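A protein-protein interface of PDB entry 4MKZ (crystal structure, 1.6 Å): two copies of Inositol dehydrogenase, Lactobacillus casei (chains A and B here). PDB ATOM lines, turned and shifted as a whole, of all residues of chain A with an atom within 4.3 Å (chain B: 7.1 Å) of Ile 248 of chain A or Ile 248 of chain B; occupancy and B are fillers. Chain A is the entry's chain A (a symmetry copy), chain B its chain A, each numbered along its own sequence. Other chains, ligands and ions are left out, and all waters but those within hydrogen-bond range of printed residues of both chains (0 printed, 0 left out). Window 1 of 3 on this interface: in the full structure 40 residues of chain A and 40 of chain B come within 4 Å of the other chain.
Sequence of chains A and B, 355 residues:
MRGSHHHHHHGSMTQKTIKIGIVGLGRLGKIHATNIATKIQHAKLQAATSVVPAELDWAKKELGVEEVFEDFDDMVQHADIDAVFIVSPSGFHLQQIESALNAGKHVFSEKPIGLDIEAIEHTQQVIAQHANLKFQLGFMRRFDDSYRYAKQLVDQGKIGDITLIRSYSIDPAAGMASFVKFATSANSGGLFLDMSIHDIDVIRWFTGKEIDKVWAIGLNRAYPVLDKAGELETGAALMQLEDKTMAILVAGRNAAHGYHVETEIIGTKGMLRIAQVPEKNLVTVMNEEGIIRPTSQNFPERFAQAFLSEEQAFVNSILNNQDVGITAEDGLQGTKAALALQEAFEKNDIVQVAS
Of the printed residues of chain B, Ile 248 of chain A touches Ile 248 (3.7 Å) and Val 250 (3.7 Å).
Of chain A, only Ile 248 and Val 250 come within 4 Å of Ile 248 of chain B.
Of the printed residues of chain A, Val 250 of chain B touches Leu 164 (3.8 Å) and Ile 248 (3.7 Å).
Of the printed residues of chain A, Leu 164 of chain B touches Val 250 (3.8 Å).
Of the printed residues of chain A, Ala 237 of chain B touches Leu 238.
Printed residues of chain B within 4 Å of Ala 237 of chain A: Leu 238 (3.9 Å).
Ser 167 of chain A touches none of the printed residues of chain B.
Asp 199 of chain B touches none of the printed residues of chain A.
The nearest residue of chain B that does not touch Ile 248 of chain A is Ala 236 of chain B (4.4 Å).
The nearest printed residue of chain A that does not touch Ile 248 of chain B is Leu 249 of chain A (4.8 Å).
Leu 164 of chain A touches Val 250 of chain B, and with the chains exchanged Val 250 of chain A touches Leu 164 of chain B.
Arg 166 of chain A touches its own counterpart, Arg 166 of chain B.
Ile 248 of chain B touches its own counterpart, Ile 248 of chain A.
Ile 248 of chain A touches Val 250 of chain B, and with the chains exchanged Val 250 of chain A touches Ile 248 of chain B.
Among the printed residues, merely in contact across the chains: Arg 166 of chain A with Arg 166 of chain B (3.5 Å), Ile 248 of chain A with Ile 248 of chain B (3.7 Å), Ile 248 of chain A with Val 250 of chain B (3.7 Å), Val 250 of chain A with Ile 248 of chain B (3.7 Å), Leu 238 of chain A with Leu 238 of chain B (3.8 Å), Val 250 of chain A with Leu 164 of chain B (3.8 Å), Leu 164 of chain A with Val 250 of chain B (3.8 Å), Leu 238 of chain A with Ala 236 of chain B (3.8 Å), Leu 164 of chain A with Ala 236 of chain B (3.8 Å), Ala 237 of chain A with Leu 238 of chain B (3.9 Å) and Leu 238 of chain A with Ala 237 of chain B (3.9 Å).
Among the printed residues, 12 pairs touch across the chains.
The backbone carbonyl oxygen (O) of Ser 167 of chain B is in hydrogen-bond range of the backbone NH (N) of Val 250 of chain B (3.1 Å).
The backbone NH (N) of Ala 237 of chain B lies within hydrogen-bond range of the backbone carbonyl oxygen (O) of Leu 249 of chain B, at 2.9 Å.
The backbone carbonyl oxygen (O) of Ile 165 of chain A lies within hydrogen-bond range of the backbone NH (N) of Ile 248 of chain A (2.8 Å).
N of Ser 167 of chain A sits at hydrogen-bond distance from O of Ile 248 of chain A (2.9 Å).
O of Ser 167 of chain A is in hydrogen-bond range of N of Val 250 of chain A, at 3.1 Å.
O of Leu 249 of chain A lies within hydrogen-bond range of N of Ala 237 of chain A (2.9 Å).
The side-chain hydroxyl of Tyr 168 of chain B sits at hydrogen-bond distance from the guanidinium group of Arg 166 of chain A (3.2 Å).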
ATOM      1  N   LEU A 164     -22.108 -18.331 -25.101  1.00  0.00           N
ATOM      2  CA  LEU A 164     -21.027 -18.046 -24.167  1.00  0.00           C
ATOM      3  C   LEU A 164     -21.003 -19.070 -23.045  1.00  0.00           C
ATOM      4  O   LEU A 164     -22.054 -19.482 -22.545  1.00  0.00           O
ATOM      5  CB  LEU A 164     -21.202 -16.630 -23.587  1.00  0.00           C
ATOM      6  CG  LEU A 164     -20.145 -16.113 -22.599  1.00  0.00           C
ATOM      7  CD1 LEU A 164     -20.019 -14.599 -22.733  1.00  0.00           C
ATOM      8  CD2 LEU A 164     -20.513 -16.454 -21.160  1.00  0.00           C
ATOM      9  N   ILE A 165     -19.802 -19.476 -22.649  1.00  0.00           N
ATOM     10  CA  ILE A 165     -19.652 -20.290 -21.457  1.00  0.00           C
ATOM     11  C   ILE A 165     -18.710 -19.580 -20.500  1.00  0.00           C
ATOM     12  O   ILE A 165     -17.643 -19.133 -20.894  1.00  0.00           O
ATOM     13  CB  ILE A 165     -19.110 -21.704 -21.774  1.00  0.00           C
ATOM     14  CG1 ILE A 165     -20.163 -22.491 -22.549  1.00  0.00           C
ATOM     15  CG2 ILE A 165     -18.761 -22.433 -20.489  1.00  0.00           C
ATOM     16  CD1 ILE A 165     -19.713 -23.853 -22.994  1.00  0.00           C
ATOM     17  N   ARG A 166     -19.126 -19.457 -19.241  1.00  0.00           N
ATOM     18  CA  ARG A 166     -18.259 -18.902 -18.207  1.00  0.00           C
ATOM     19  C   ARG A 166     -18.011 -20.001 -17.201  1.00  0.00           C
ATOM     20  O   ARG A 166     -18.951 -20.625 -16.712  1.00  0.00           O
ATOM     21  CB  ARG A 166     -18.913 -17.704 -17.507  1.00  0.00           C
ATOM     22  CG  ARG A 166     -18.156 -17.266 -16.242  1.00  0.00           C
ATOM     23  CD  ARG A 166     -18.802 -16.070 -15.543  1.00  0.00           C
ATOM     24  NE  ARG A 166     -20.133 -16.359 -15.009  1.00  0.00           N
ATOM     25  CZ  ARG A 166     -20.376 -16.983 -13.861  1.00  0.00           C
ATOM     26  NH1 ARG A 166     -19.376 -17.413 -13.099  1.00  0.00           N
ATOM     27  NH2 ARG A 166     -21.629 -17.203 -13.484  1.00  0.00           N
ATOM     28  N   SER A 167     -16.748 -20.263 -16.900  1.00  0.00           N
ATOM     29  CA  SER A 167     -16.450 -21.331 -15.960  1.00  0.00           C
ATOM     30  C   SER A 167     -15.417 -20.874 -14.946  1.00  0.00           C
ATOM     31  O   SER A 167     -14.405 -20.282 -15.305  1.00  0.00           O
ATOM     32  CB  SER A 167     -15.993 -22.600 -16.704  1.00  0.00           C
ATOM     33  OG  SER A 167     -16.331 -23.769 -15.964  1.00  0.00           O
ATOM     34  N   ALA A 237      -9.570 -15.060 -17.854  1.00  0.00           N
ATOM     35  CA  ALA A 237      -9.289 -15.162 -19.275  1.00  0.00           C
ATOM     36  C   ALA A 237     -10.523 -15.017 -20.133  1.00  0.00           C
ATOM     37  O   ALA A 237     -11.620 -15.396 -19.734  1.00  0.00           O
ATOM     38  CB  ALA A 237      -8.591 -16.488 -19.574  1.00  0.00           C
ATOM     39  N   LEU A 238     -10.324 -14.451 -21.320  1.00  0.00           N
ATOM     40  CA  LEU A 238     -11.358 -14.392 -22.337  1.00  0.00           C
ATOM     41  C   LEU A 238     -10.878 -15.239 -23.505  1.00  0.00           C
ATOM     42  O   LEU A 238      -9.706 -15.189 -23.878  1.00  0.00           O
ATOM     43  CB  LEU A 238     -11.584 -12.944 -22.781  1.00  0.00           C
ATOM     44  CG  LEU A 238     -12.673 -12.692 -23.823  1.00  0.00           C
ATOM     45  CD1 LEU A 238     -14.043 -13.147 -23.311  1.00  0.00           C
ATOM     46  CD2 LEU A 238     -12.706 -11.201 -24.191  1.00  0.00           C
ATOM     47  N   ALA A 247     -15.944 -17.545 -24.476  1.00  0.00           N
ATOM     48  CA  ALA A 247     -15.769 -18.230 -23.205  1.00  0.00           C
ATOM     49  C   ALA A 247     -14.994 -17.356 -22.240  1.00  0.00           C
ATOM     50  O   ALA A 247     -14.120 -16.588 -22.635  1.00  0.00           O
ATOM     51  CB  ALA A 247     -15.078 -19.583 -23.397  1.00  0.00           C
ATOM     52  N   ILE A 248     -15.347 -17.469 -20.963  1.00  0.00           N
ATOM     53  CA  ILE A 248     -14.694 -16.720 -19.904  1.00  0.00           C
ATOM     54  C   ILE A 248     -14.244 -17.693 -18.844  1.00  0.00           C
ATOM     55  O   ILE A 248     -15.015 -18.569 -18.441  1.00  0.00           O
ATOM     56  CB  ILE A 248     -15.675 -15.729 -19.239  1.00  0.00           C
ATOM     57  CG1 ILE A 248     -16.145 -14.683 -20.251  1.00  0.00           C
ATOM     58  CG2 ILE A 248     -15.020 -15.059 -18.036  1.00  0.00           C
ATOM     59  CD1 ILE A 248     -17.324 -13.860 -19.783  1.00  0.00           C
ATOM     60  N   LEU A 249     -13.003 -17.550 -18.390  1.00  0.00           N
ATOM     61  CA  LEU A 249     -12.495 -18.380 -17.307  1.00  0.00           C
ATOM     62  C   LEU A 249     -12.087 -17.520 -16.122  1.00  0.00           C
ATOM     63  O   LEU A 249     -11.548 -16.443 -16.301  1.00  0.00           O
ATOM     64  CB  LEU A 249     -11.277 -19.180 -17.766  1.00  0.00           C
ATOM     65  CG  LEU A 249     -11.473 -20.188 -18.891  1.00  0.00           C
ATOM     66  CD1 LEU A 249     -10.156 -20.905 -19.211  1.00  0.00           C
ATOM     67  CD2 LEU A 249     -12.541 -21.190 -18.479  1.00  0.00           C
ATOM     68  N   VAL A 250     -12.342 -18.004 -14.916  1.00  0.00           N
ATOM     69  CA  VAL A 250     -11.659 -17.470 -13.748  1.00  0.00           C
ATOM     70  C   VAL A 250     -11.052 -18.657 -13.021  1.00  0.00           C
ATOM     71  O   VAL A 250     -11.695 -19.701 -12.884  1.00  0.00           O
ATOM     72  CB  VAL A 250     -12.588 -16.676 -12.817  1.00  0.00           C
ATOM     73  CG1 VAL A 250     -11.878 -16.389 -11.491  1.00  0.00           C
ATOM     74  CG2 VAL A 250     -13.000 -15.383 -13.473  1.00  0.00           C
ATOM     75  N   LEU B 164     -11.340  -8.844  -8.501  1.00  0.00           N
ATOM     76  CA  LEU B 164     -12.028  -8.974  -9.778  1.00  0.00           C
ATOM     77  C   LEU B 164     -13.469  -8.509  -9.661  1.00  0.00           C
ATOM     78  O   LEU B 164     -14.138  -8.774  -8.659  1.00  0.00           O
ATOM     79  CB  LEU B 164     -11.982 -10.441 -10.245  1.00  0.00           C
ATOM     80  CG  LEU B 164     -12.625 -10.795 -11.595  1.00  0.00           C
ATOM     81  CD1 LEU B 164     -11.876 -11.965 -12.225  1.00  0.00           C
ATOM     82  CD2 LEU B 164     -14.091 -11.177 -11.431  1.00  0.00           C
ATOM     83  N   ILE B 165     -13.945  -7.817 -10.690  1.00  0.00           N
ATOM     84  CA  ILE B 165     -15.359  -7.501 -10.778  1.00  0.00           C
ATOM     85  C   ILE B 165     -15.900  -8.052 -12.087  1.00  0.00           C
ATOM     86  O   ILE B 165     -15.312  -7.848 -13.138  1.00  0.00           O
ATOM     87  CB  ILE B 165     -15.629  -5.979 -10.700  1.00  0.00           C
ATOM     88  CG1 ILE B 165     -15.290  -5.474  -9.300  1.00  0.00           C
ATOM     89  CG2 ILE B 165     -17.083  -5.685 -11.019  1.00  0.00           C
ATOM     90  CD1 ILE B 165     -15.425  -3.987  -9.130  1.00  0.00           C
ATOM     91  N   ARG B 166     -17.014  -8.778 -12.008  1.00  0.00           N
ATOM     92  CA  ARG B 166     -17.691  -9.258 -13.209  1.00  0.00           C
ATOM     93  C   ARG B 166     -19.047  -8.597 -13.245  1.00  0.00           C
ATOM     94  O   ARG B 166     -19.789  -8.635 -12.265  1.00  0.00           O
ATOM     95  CB  ARG B 166     -17.864 -10.782 -13.185  1.00  0.00           C
ATOM     96  CG  ARG B 166     -18.804 -11.292 -14.290  1.00  0.00           C
ATOM     97  CD  ARG B 166     -18.977 -12.811 -14.275  1.00  0.00           C
ATOM     98  NE  ARG B 166     -19.638 -13.307 -13.067  1.00  0.00           N
ATOM     99  CZ  ARG B 166     -20.950 -13.296 -12.856  1.00  0.00           C
ATOM    100  NH1 ARG B 166     -21.778 -12.798 -13.768  1.00  0.00           N
ATOM    101  NH2 ARG B 166     -21.437 -13.761 -11.713  1.00  0.00           N
ATOM    102  N   SER B 167     -19.376  -7.966 -14.363  1.00  0.00           N
ATOM    103  CA  SER B 167     -20.658  -7.286 -14.444  1.00  0.00           C
ATOM    104  C   SER B 167     -21.350  -7.608 -15.756  1.00  0.00           C
ATOM    105  O   SER B 167     -20.737  -7.561 -16.816  1.00  0.00           O
ATOM    106  CB  SER B 167     -20.482  -5.767 -14.252  1.00  0.00           C
ATOM    107  OG  SER B 167     -21.650  -5.192 -13.677  1.00  0.00           O
ATOM    108  N   TYR B 168     -22.636  -7.935 -15.666  1.00  0.00           N
ATOM    109  CA  TYR B 168     -23.432  -8.340 -16.812  1.00  0.00           C
ATOM    110  C   TYR B 168     -24.561  -7.353 -16.955  1.00  0.00           C
ATOM    111  O   TYR B 168     -25.214  -7.030 -15.970  1.00  0.00           O
ATOM    112  CB  TYR B 168     -24.097  -9.693 -16.537  1.00  0.00           C
ATOM    113  CG  TYR B 168     -23.271 -10.936 -16.749  1.00  0.00           C
ATOM    114  CD1 TYR B 168     -21.887 -10.901 -16.793  1.00  0.00           C
ATOM    115  CD2 TYR B 168     -23.902 -12.165 -16.901  1.00  0.00           C
ATOM    116  CE1 TYR B 168     -21.154 -12.072 -16.986  1.00  0.00           C
ATOM    117  CE2 TYR B 168     -23.176 -13.336 -17.088  1.00  0.00           C
ATOM    118  CZ  TYR B 168     -21.810 -13.276 -17.137  1.00  0.00           C
ATOM    119  OH  TYR B 168     -21.079 -14.423 -17.335  1.00  0.00           O
ATOM    120  N   ASP B 199     -21.854  -0.402 -16.146  1.00  0.00           N
ATOM    121  CA  ASP B 199     -20.951  -1.385 -15.575  1.00  0.00           C
ATOM    122  C   ASP B 199     -19.562  -0.792 -15.381  1.00  0.00           C
ATOM    123  O   ASP B 199     -18.937  -0.977 -14.333  1.00  0.00           O
ATOM    124  CB  ASP B 199     -20.866  -2.616 -16.486  1.00  0.00           C
ATOM    125  CG  ASP B 199     -22.182  -3.350 -16.592  1.00  0.00           C
ATOM    126  OD1 ASP B 199     -22.760  -3.685 -15.539  1.00  0.00           O
ATOM    127  OD2 ASP B 199     -22.640  -3.592 -17.728  1.00  0.00           O
ATOM    128  N   ILE B 203     -17.602  -0.297 -11.820  1.00  0.00           N
ATOM    129  CA  ILE B 203     -16.239  -0.777 -11.593  1.00  0.00           C
ATOM    130  C   ILE B 203     -15.373   0.353 -11.017  1.00  0.00           C
ATOM    131  O   ILE B 203     -14.708   0.175  -9.989  1.00  0.00           O
ATOM    132  CB  ILE B 203     -15.637  -1.360 -12.883  1.00  0.00           C
ATOM    133  CG1 ILE B 203     -16.322  -2.690 -13.215  1.00  0.00           C
ATOM    134  CG2 ILE B 203     -14.137  -1.584 -12.733  1.00  0.00           C
ATOM    135  CD1 ILE B 203     -16.135  -3.137 -14.642  1.00  0.00           C
ATOM    136  N   GLY B 235     -21.897  -9.631 -26.362  1.00  0.00           N
ATOM    137  CA  GLY B 235     -20.473  -9.368 -26.381  1.00  0.00           C
ATOM    138  C   GLY B 235     -19.883  -9.654 -25.020  1.00  0.00           C
ATOM    139  O   GLY B 235     -20.600  -9.698 -24.018  1.00  0.00           O
ATOM    140  N   ALA B 236     -18.578  -9.868 -24.981  1.00  0.00           N
ATOM    141  CA  ALA B 236     -17.897 -10.108 -23.729  1.00  0.00           C
ATOM    142  C   ALA B 236     -16.547  -9.417 -23.748  1.00  0.00           C
ATOM    143  O   ALA B 236     -15.935  -9.246 -24.810  1.00  0.00           O
ATOM    144  CB  ALA B 236     -17.731 -11.600 -23.485  1.00  0.00           C
ATOM    145  N   ALA B 237     -16.066  -9.038 -22.573  1.00  0.00           N
ATOM    146  CA  ALA B 237     -14.802  -8.327 -22.502  1.00  0.00           C
ATOM    147  C   ALA B 237     -14.013  -8.647 -21.256  1.00  0.00           C
ATOM    148  O   ALA B 237     -14.579  -8.923 -20.202  1.00  0.00           O
ATOM    149  CB  ALA B 237     -15.044  -6.821 -22.602  1.00  0.00           C
ATOM    150  N   LEU B 238     -12.691  -8.615 -21.397  1.00  0.00           N
ATOM    151  CA  LEU B 238     -11.785  -8.723 -20.269  1.00  0.00           C
ATOM    152  C   LEU B 238     -11.048  -7.397 -20.164  1.00  0.00           C
ATOM    153  O   LEU B 238     -10.638  -6.824 -21.173  1.00  0.00           O
ATOM    154  CB  LEU B 238     -10.795  -9.871 -20.492  1.00  0.00           C
ATOM    155  CG  LEU B 238      -9.788 -10.155 -19.378  1.00  0.00           C
ATOM    156  CD1 LEU B 238     -10.500 -10.520 -18.072  1.00  0.00           C
ATOM    157  CD2 LEU B 238      -8.842 -11.287 -19.808  1.00  0.00           C
ATOM    158  N   MET B 239     -10.915  -6.897 -18.945  1.00  0.00           N
ATOM    159  CA  MET B 239     -10.272  -5.611 -18.720  1.00  0.00           C
ATOM    160  C   MET B 239      -9.257  -5.706 -17.595  1.00  0.00           C
ATOM    161  O   MET B 239      -9.508  -6.325 -16.564  1.00  0.00           O
ATOM    162  CB  MET B 239     -11.325  -4.543 -18.405  1.00  0.00           C
ATOM    163  CG  MET B 239     -12.493  -4.519 -19.381  1.00  0.00           C
ATOM    164  SD  MET B 239     -13.533  -3.060 -19.249  1.00  0.00           S
ATOM    165  CE  MET B 239     -14.233  -3.274 -17.625  1.00  0.00           C
ATOM    166  N   LEU B 241      -7.150  -3.521 -14.882  1.00  0.00           N
ATOM    167  CA  LEU B 241      -7.135  -2.191 -14.250  1.00  0.00           C
ATOM    168  C   LEU B 241      -5.706  -1.780 -13.849  1.00  0.00           C
ATOM    169  O   LEU B 241      -4.773  -2.574 -13.962  1.00  0.00           O
ATOM    170  CB  LEU B 241      -8.084  -2.138 -13.052  1.00  0.00           C
ATOM    171  CG  LEU B 241      -9.570  -1.900 -13.346  1.00  0.00           C
ATOM    172  CD1 LEU B 241     -10.166  -2.980 -14.232  1.00  0.00           C
ATOM    173  CD2 LEU B 241     -10.353  -1.790 -12.048  1.00  0.00           C
ATOM    174  N   MET B 246      -8.758  -7.072 -12.042  1.00  0.00           N
ATOM    175  CA  MET B 246      -9.345  -7.631 -13.238  1.00  0.00           C
ATOM    176  C   MET B 246     -10.812  -7.300 -13.309  1.00  0.00           C
ATOM    177  O   MET B 246     -11.475  -7.162 -12.285  1.00  0.00           O
ATOM    178  CB  MET B 246      -9.156  -9.143 -13.217  1.00  0.00           C
ATOM    179  CG  MET B 246      -7.706  -9.519 -13.126  1.00  0.00           C
ATOM    180  SD  MET B 246      -7.421 -11.281 -12.893  1.00  0.00           S
ATOM    181  CE  MET B 246      -7.808 -11.492 -11.163  1.00  0.00           C
ATOM    182  N   ALA B 247     -11.325  -7.195 -14.524  1.00  0.00           N
ATOM    183  CA  ALA B 247     -12.756  -7.006 -14.697  1.00  0.00           C
ATOM    184  C   ALA B 247     -13.244  -7.767 -15.914  1.00  0.00           C
ATOM    185  O   ALA B 247     -12.531  -7.909 -16.905  1.00  0.00           O
ATOM    186  CB  ALA B 247     -13.108  -5.519 -14.802  1.00  0.00           C
ATOM    187  N   ILE B 248     -14.469  -8.275 -15.812  1.00  0.00           N
ATOM    188  CA  ILE B 248     -15.098  -9.015 -16.893  1.00  0.00           C
ATOM    189  C   ILE B 248     -16.444  -8.394 -17.169  1.00  0.00           C
ATOM    190  O   ILE B 248     -17.203  -8.122 -16.235  1.00  0.00           O
ATOM    191  CB  ILE B 248     -15.338 -10.487 -16.490  1.00  0.00           C
ATOM    192  CG1 ILE B 248     -14.006 -11.194 -16.231  1.00  0.00           C
ATOM    193  CG2 ILE B 248     -16.131 -11.212 -17.572  1.00  0.00           C
ATOM    194  CD1 ILE B 248     -14.145 -12.535 -15.547  1.00  0.00           C
ATOM    195  N   LEU B 249     -16.746  -8.168 -18.443  1.00  0.00           N
ATOM    196  CA  LEU B 249     -18.051  -7.652 -18.829  1.00  0.00           C
ATOM    197  C   LEU B 249     -18.760  -8.631 -19.752  1.00  0.00           C
ATOM    198  O   LEU B 249     -18.132  -9.248 -20.593  1.00  0.00           O
ATOM    199  CB  LEU B 249     -17.911  -6.316 -19.558  1.00  0.00           C
ATOM    200  CG  LEU B 249     -17.307  -5.149 -18.788  1.00  0.00           C
ATOM    201  CD1 LEU B 249     -17.255  -3.892 -19.666  1.00  0.00           C
ATOM    202  CD2 LEU B 249     -18.140  -4.894 -17.540  1.00  0.00           C
ATOM    203  N   VAL B 250     -20.069  -8.762 -19.592  1.00  0.00           N
ATOM    204  CA  VAL B 250     -20.884  -9.349 -20.644  1.00  0.00           C
ATOM    205  C   VAL B 250     -22.007  -8.365 -20.920  1.00  0.00           C
ATOM    206  O   VAL B 250     -22.589  -7.803 -19.988  1.00  0.00           O
ATOM    207  CB  VAL B 250     -21.445 -10.730 -20.273  1.00  0.00           C
ATOM    208  CG1 VAL B 250     -22.505 -11.155 -21.293  1.00  0.00           C
ATOM    209  CG2 VAL B 250     -20.334 -11.747 -20.227  1.00  0.00           C
ATOM    210  N   GLU B 264     -20.769  -8.953  -9.758  1.00  0.00           N
ATOM    211  CA  GLU B 264     -20.046  -9.794  -8.826  1.00  0.00           C
ATOM    212  C   GLU B 264     -18.745  -9.101  -8.462  1.00  0.00           C
ATOM    213  O   GLU B 264     -18.038  -8.587  -9.333  1.00  0.00           O
ATOM    214  CB  GLU B 264     -19.743 -11.119  -9.511  1.00  0.00           C
ATOM    215  CG  GLU B 264     -18.731 -11.984  -8.834  1.00  0.00           C
ATOM    216  CD  GLU B 264     -18.330 -13.109  -9.749  1.00  0.00           C
ATOM    217  OE1 GLU B 264     -19.158 -14.033  -9.936  1.00  0.00           O
ATOM    218  OE2 GLU B 264     -17.220 -13.047 -10.317  1.00  0.00           O
